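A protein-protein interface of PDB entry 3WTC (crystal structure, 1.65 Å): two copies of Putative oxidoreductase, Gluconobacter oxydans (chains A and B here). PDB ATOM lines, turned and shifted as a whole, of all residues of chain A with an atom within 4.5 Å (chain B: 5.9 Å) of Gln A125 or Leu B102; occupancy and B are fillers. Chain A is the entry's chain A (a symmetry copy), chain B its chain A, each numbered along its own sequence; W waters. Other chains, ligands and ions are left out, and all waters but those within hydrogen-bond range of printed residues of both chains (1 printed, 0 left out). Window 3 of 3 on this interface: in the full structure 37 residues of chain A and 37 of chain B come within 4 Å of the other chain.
O of Leu B102 touches NH2 of Arg A69, at 3.6 Å. NH1 of Arg A69 touches CG of Glu B105, at 3.98 Å. Leu A121 touches Ile B101 (CD1 to CG2, 3.9 Å). Leu A121 touches Ile B104. O of Ile B104 touches CZ3 of Trp A122, 3.4 Å away. Glu B105 touches Trp A122 (C to CH2, 3.8 Å). Ala A128 touches Leu B102 (CB to CD2, 3.7 Å). Lys A132 touches Leu B102.
Water W1 lies within hydrogen-bond range of NH2 of Arg A69 (2.9 Å), O of Asp B103 (3.4 Å) and OE1 of Glu B105 (3.5 Å).
The side-chain hydroxyl (OG1) of Thr A129 is in hydrogen-bond range of the backbone carbonyl oxygen (O) of Gln A125, 2.8 Å away. The guanidinium group (NE) of Arg A69 is in hydrogen-bond range of the side-chain amide oxygen (OE1) of Gln A125.
Printed residues of chain B within 4 Å of Arg A69: Leu B102 (3.6 Å), Ile B104 (3.3 Å) and Glu B105 (3.98 Å). Gln A125 touches just these residues of chain B: Ile B101 (2.8 Å), Leu B102 (3.4 Å) and Ile B104 (3.0 Å). Of the printed residues of chain B, Lys A132 touches Leu B102. Leu A176 touches none of the printed residues of chain B. Of chain A, only Arg A69 (3.6 Å), Gln A125 (3.4 Å), Ala A128 (3.7 Å) and Lys A132 (3.7 Å) come within 4 Å of Leu B102. Of the printed residues of chain A, Glu B105 touches Arg A69 (3.98 Å) and Trp A122 (3.8 Å). The nearest residue of chain B that does not touch Gln A125 is Asp B103 (4.1 Å).
Hydrophobic or aromatic side chains of chain A within 4 Å of the printed part of chain B: Leu A121, Trp A122 and Ala A128. Printed residues of chain B that touch a printed residue of chain A: Ile B101, Leu B102, Ile B104 and Glu B105. Hydrophobic or aromatic side chains of chain B within 4 Å of the printed part of chain A: Ile B101, Leu B102 and Ile B104.
The backbone carbonyl oxygen (O) of Ile B104 is in hydrogen-bond range of the guanidinium group (NH2) of Arg A69 (3.3 Å). The backbone carbonyl oxygen (O) of Ile B104 sits at hydrogen-bond distance from the side-chain amide nitrogen (NE2) of Gln A125 (3.0 Å). The side-chain amide nitrogen (NE2) of Gln A125 sits at hydrogen-bond distance from the backbone carbonyl oxygen (O) of Ile B101 (2.8 Å). O of Leu B102 lies within hydrogen-bond range of NE2 of Gln A125, at 3.4 Å.
No position is printed for both chains. Of the 12 pairs that touch across the chains among the printed residues, none has its exchanged pair printed and touching as well.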
ATOM      1  N   ARG A  69     -10.489  11.047 -26.775  1.00  0.00           N
ATOM      2  CA  ARG A  69     -11.153  12.274 -26.319  1.00  0.00           C
ATOM      3  C   ARG A  69     -10.186  13.376 -25.981  1.00  0.00           C
ATOM      4  O   ARG A  69     -10.262  14.494 -26.481  1.00  0.00           O
ATOM      5  CB  ARG A  69     -12.039  11.995 -25.110  1.00  0.00           C
ATOM      6  CG  ARG A  69     -12.782  13.140 -24.564  1.00  0.00           C
ATOM      7  CD  ARG A  69     -13.702  12.664 -23.458  1.00  0.00           C
ATOM      8  NE  ARG A  69     -14.537  13.717 -22.955  1.00  0.00           N
ATOM      9  CZ  ARG A  69     -14.597  14.190 -21.718  1.00  0.00           C
ATOM     10  NH1 ARG A  69     -13.822  13.670 -20.783  1.00  0.00           N
ATOM     11  NH2 ARG A  69     -15.500  15.124 -21.428  1.00  0.00           N
ATOM     12  N   LEU A 121     -18.663  12.384 -31.069  1.00  0.00           N
ATOM     13  CA  LEU A 121     -18.885  13.050 -29.776  1.00  0.00           C
ATOM     14  C   LEU A 121     -17.605  13.798 -29.327  1.00  0.00           C
ATOM     15  O   LEU A 121     -17.713  14.949 -28.876  1.00  0.00           O
ATOM     16  CB  LEU A 121     -19.271  12.024 -28.746  1.00  0.00           C
ATOM     17  CG  LEU A 121     -19.636  12.600 -27.392  1.00  0.00           C
ATOM     18  CD1 LEU A 121     -20.628  13.717 -27.430  1.00  0.00           C
ATOM     19  CD2 LEU A 121     -20.119  11.474 -26.492  1.00  0.00           C
ATOM     20  N   TRP A 122     -16.459  13.152 -29.481  1.00  0.00           N
ATOM     21  CA  TRP A 122     -15.217  13.834 -28.997  1.00  0.00           C
ATOM     22  C   TRP A 122     -14.921  15.076 -29.821  1.00  0.00           C
ATOM     23  O   TRP A 122     -14.374  16.082 -29.324  1.00  0.00           O
ATOM     24  CB  TRP A 122     -14.001  12.917 -28.928  1.00  0.00           C
ATOM     25  CG  TRP A 122     -14.191  11.634 -28.150  1.00  0.00           C
ATOM     26  CD1 TRP A 122     -13.533  10.492 -28.412  1.00  0.00           C
ATOM     27  CD2 TRP A 122     -15.057  11.375 -27.023  1.00  0.00           C
ATOM     28  NE1 TRP A 122     -13.904   9.537 -27.480  1.00  0.00           N
ATOM     29  CE2 TRP A 122     -14.846  10.051 -26.644  1.00  0.00           C
ATOM     30  CE3 TRP A 122     -15.941  12.156 -26.272  1.00  0.00           C
ATOM     31  CZ2 TRP A 122     -15.565   9.447 -25.562  1.00  0.00           C
ATOM     32  CZ3 TRP A 122     -16.653  11.576 -25.179  1.00  0.00           C
ATOM     33  CH2 TRP A 122     -16.434  10.245 -24.853  1.00  0.00           C
ATOM     34  N   GLY A 123     -15.228  15.013 -31.127  1.00  0.00           N
ATOM     35  CA  GLY A 123     -15.094  16.201 -31.945  1.00  0.00           C
ATOM     36  C   GLY A 123     -16.015  17.331 -31.634  1.00  0.00           C
ATOM     37  O   GLY A 123     -15.626  18.474 -31.602  1.00  0.00           O
ATOM     38  N   MET A 124     -17.283  17.006 -31.431  1.00  0.00           N
ATOM     39  CA  MET A 124     -18.235  17.952 -30.942  1.00  0.00           C
ATOM     40  C   MET A 124     -17.718  18.605 -29.635  1.00  0.00           C
ATOM     41  O   MET A 124     -17.791  19.790 -29.471  1.00  0.00           O
ATOM     42  CB  MET A 124     -19.615  17.335 -30.676  1.00  0.00           C
ATOM     43  CG  MET A 124     -20.253  16.874 -31.936  1.00  0.00           C
ATOM     44  SD  MET A 124     -22.120  17.001 -31.803  1.00  0.00           S
ATOM     45  CE  MET A 124     -22.018  15.415 -31.210  1.00  0.00           C
ATOM     46  N   GLN A 125     -17.328  17.768 -28.656  1.00  0.00           N
ATOM     47  CA  GLN A 125     -16.798  18.320 -27.410  1.00  0.00           C
ATOM     48  C   GLN A 125     -15.573  19.225 -27.620  1.00  0.00           C
ATOM     49  O   GLN A 125     -15.493  20.302 -27.039  1.00  0.00           O
ATOM     50  CB  GLN A 125     -16.471  17.226 -26.448  1.00  0.00           C
ATOM     51  CG  GLN A 125     -17.617  16.487 -25.869  1.00  0.00           C
ATOM     52  CD  GLN A 125     -17.207  15.432 -24.900  1.00  0.00           C
ATOM     53  OE1 GLN A 125     -16.051  15.176 -24.672  1.00  0.00           O
ATOM     54  NE2 GLN A 125     -18.218  14.862 -24.237  1.00  0.00           N
ATOM     55  N   ALA A 126     -14.618  18.796 -28.419  1.00  0.00           N
ATOM     56  CA  ALA A 126     -13.343  19.555 -28.670  1.00  0.00           C
ATOM     57  C   ALA A 126     -13.712  20.894 -29.287  1.00  0.00           C
ATOM     58  O   ALA A 126     -13.120  21.941 -28.938  1.00  0.00           O
ATOM     59  CB  ALA A 126     -12.412  18.786 -29.552  1.00  0.00           C
ATOM     60  N   ALA A 127     -14.593  20.917 -30.273  1.00  0.00           N
ATOM     61  CA  ALA A 127     -14.880  22.174 -30.941  1.00  0.00           C
ATOM     62  C   ALA A 127     -15.753  23.077 -30.074  1.00  0.00           C
ATOM     63  O   ALA A 127     -15.495  24.273 -30.024  1.00  0.00           O
ATOM     64  CB  ALA A 127     -15.599  21.925 -32.256  1.00  0.00           C
ATOM     65  N   ALA A 128     -16.797  22.554 -29.407  1.00  0.00           N
ATOM     66  CA  ALA A 128     -17.679  23.389 -28.632  1.00  0.00           C
ATOM     67  C   ALA A 128     -16.903  23.976 -27.428  1.00  0.00           C
ATOM     68  O   ALA A 128     -17.170  25.096 -27.075  1.00  0.00           O
ATOM     69  CB  ALA A 128     -18.858  22.589 -28.111  1.00  0.00           C
ATOM     70  N   THR A 129     -15.948  23.240 -26.914  1.00  0.00           N
ATOM     71  CA  THR A 129     -15.098  23.769 -25.795  1.00  0.00           C
ATOM     72  C   THR A 129     -14.384  25.005 -26.296  1.00  0.00           C
ATOM     73  O   THR A 129     -14.352  26.027 -25.610  1.00  0.00           O
ATOM     74  CB  THR A 129     -14.130  22.697 -25.280  1.00  0.00           C
ATOM     75  OG1 THR A 129     -14.876  21.640 -24.705  1.00  0.00           O
ATOM     76  CG2 THR A 129     -13.148  23.276 -24.284  1.00  0.00           C
ATOM     77  N   LYS A 132     -16.899  27.972 -26.951  1.00  0.00           N
ATOM     78  CA  LYS A 132     -17.456  28.525 -25.730  1.00  0.00           C
ATOM     79  C   LYS A 132     -16.386  29.293 -24.997  1.00  0.00           C
ATOM     80  O   LYS A 132     -16.675  30.362 -24.523  1.00  0.00           O
ATOM     81  CB  LYS A 132     -17.997  27.491 -24.801  1.00  0.00           C
ATOM     82  CG  LYS A 132     -19.375  26.968 -25.279  1.00  0.00           C
ATOM     83  CD  LYS A 132     -19.893  25.777 -24.538  1.00  0.00           C
ATOM     84  CE  LYS A 132     -20.243  26.116 -23.106  1.00  0.00           C
ATOM     85  NZ  LYS A 132     -21.257  27.220 -23.042  1.00  0.00           N
ATOM     86  N   LEU A 176     -26.638  23.271 -27.069  1.00  0.00           N
ATOM     87  CA  LEU A 176     -25.642  24.250 -27.434  1.00  0.00           C
ATOM     88  C   LEU A 176     -26.233  25.490 -28.051  1.00  0.00           C
ATOM     89  O   LEU A 176     -25.472  26.456 -28.247  1.00  0.00           O
ATOM     90  CB  LEU A 176     -24.579  23.611 -28.308  1.00  0.00           C
ATOM     91  CG  LEU A 176     -23.772  22.463 -27.699  1.00  0.00           C
ATOM     92  CD1 LEU A 176     -22.813  21.914 -28.741  1.00  0.00           C
ATOM     93  CD2 LEU A 176     -23.062  22.931 -26.437  1.00  0.00           C
ATOM     94  N   PRO B 100     -24.789  16.237 -19.617  1.00  0.00           N
ATOM     95  CA  PRO B 100     -24.717  17.109 -20.785  1.00  0.00           C
ATOM     96  C   PRO B 100     -23.749  16.588 -21.821  1.00  0.00           C
ATOM     97  O   PRO B 100     -22.755  15.961 -21.450  1.00  0.00           O
ATOM     98  CB  PRO B 100     -24.196  18.417 -20.229  1.00  0.00           C
ATOM     99  CG  PRO B 100     -24.436  18.386 -18.846  1.00  0.00           C
ATOM    100  CD  PRO B 100     -24.466  16.959 -18.392  1.00  0.00           C
ATOM    101  N   ILE B 101     -24.014  16.904 -23.097  1.00  0.00           N
ATOM    102  CA  ILE B 101     -23.207  16.436 -24.209  1.00  0.00           C
ATOM    103  C   ILE B 101     -21.730  16.713 -23.946  1.00  0.00           C
ATOM    104  O   ILE B 101     -20.877  15.860 -24.207  1.00  0.00           O
ATOM    105  CB  ILE B 101     -23.643  17.042 -25.587  1.00  0.00           C
ATOM    106  CG1 ILE B 101     -24.856  16.362 -26.215  1.00  0.00           C
ATOM    107  CG2 ILE B 101     -22.506  16.978 -26.614  1.00  0.00           C
ATOM    108  CD1 ILE B 101     -24.677  15.022 -26.824  1.00  0.00           C
ATOM    109  N   LEU B 102     -21.434  17.897 -23.438  1.00  0.00           N
ATOM    110  CA  LEU B 102     -20.035  18.307 -23.250  1.00  0.00           C
ATOM    111  C   LEU B 102     -19.320  17.535 -22.178  1.00  0.00           C
ATOM    112  O   LEU B 102     -18.025  17.522 -22.148  1.00  0.00           O
ATOM    113  CB  LEU B 102     -19.910  19.827 -22.996  1.00  0.00           C
ATOM    114  CG  LEU B 102     -20.397  20.752 -24.076  1.00  0.00           C
ATOM    115  CD1 LEU B 102     -20.005  22.195 -23.739  1.00  0.00           C
ATOM    116  CD2 LEU B 102     -19.903  20.300 -25.454  1.00  0.00           C
ATOM    117  N   ASP B 103     -20.082  16.939 -21.257  1.00  0.00           N
ATOM    118  CA  ASP B 103     -19.485  16.296 -20.065  1.00  0.00           C
ATOM    119  C   ASP B 103     -19.435  14.769 -20.107  1.00  0.00           C
ATOM    120  O   ASP B 103     -18.943  14.086 -19.131  1.00  0.00           O
ATOM    121  CB  ASP B 103     -20.226  16.756 -18.816  1.00  0.00           C
ATOM    122  CG  ASP B 103     -20.126  18.258 -18.562  1.00  0.00           C
ATOM    123  OD1 ASP B 103     -19.088  18.865 -18.897  1.00  0.00           O
ATOM    124  OD2 ASP B 103     -21.154  18.808 -18.042  1.00  0.00           O
ATOM    125  N   ILE B 104     -19.908  14.168 -21.196  1.00  0.00           N
ATOM    126  CA  ILE B 104     -19.956  12.737 -21.301  1.00  0.00           C
ATOM    127  C   ILE B 104     -18.509  12.202 -21.400  1.00  0.00           C
ATOM    128  O   ILE B 104     -17.707  12.726 -22.149  1.00  0.00           O
ATOM    129  CB  ILE B 104     -20.746  12.270 -22.539  1.00  0.00           C
ATOM    130  CG1 ILE B 104     -22.224  12.762 -22.466  1.00  0.00           C
ATOM    131  CG2 ILE B 104     -20.581  10.793 -22.760  1.00  0.00           C
ATOM    132  CD1 ILE B 104     -22.989  12.535 -23.754  1.00  0.00           C
ATOM    133  N   GLU B 105     -18.186  11.230 -20.561  1.00  0.00           N
ATOM    134  CA  GLU B 105     -16.837  10.657 -20.511  1.00  0.00           C
ATOM    135  C   GLU B 105     -16.719   9.302 -21.178  1.00  0.00           C
ATOM    136  O   GLU B 105     -17.722   8.644 -21.426  1.00  0.00           O
ATOM    137  CB  GLU B 105     -16.418  10.534 -19.019  1.00  0.00           C
ATOM    138  CG  GLU B 105     -16.427  11.874 -18.364  1.00  0.00           C
ATOM    139  CD  GLU B 105     -16.052  11.905 -16.882  1.00  0.00           C
ATOM    140  OE1 GLU B 105     -15.212  12.727 -16.539  1.00  0.00           O
ATOM    141  OE2 GLU B 105     -16.639  11.170 -16.111  1.00  0.00           O
HETATM  142  O   HOH W   1     -15.836  15.475 -18.605  1.00  0.00           O
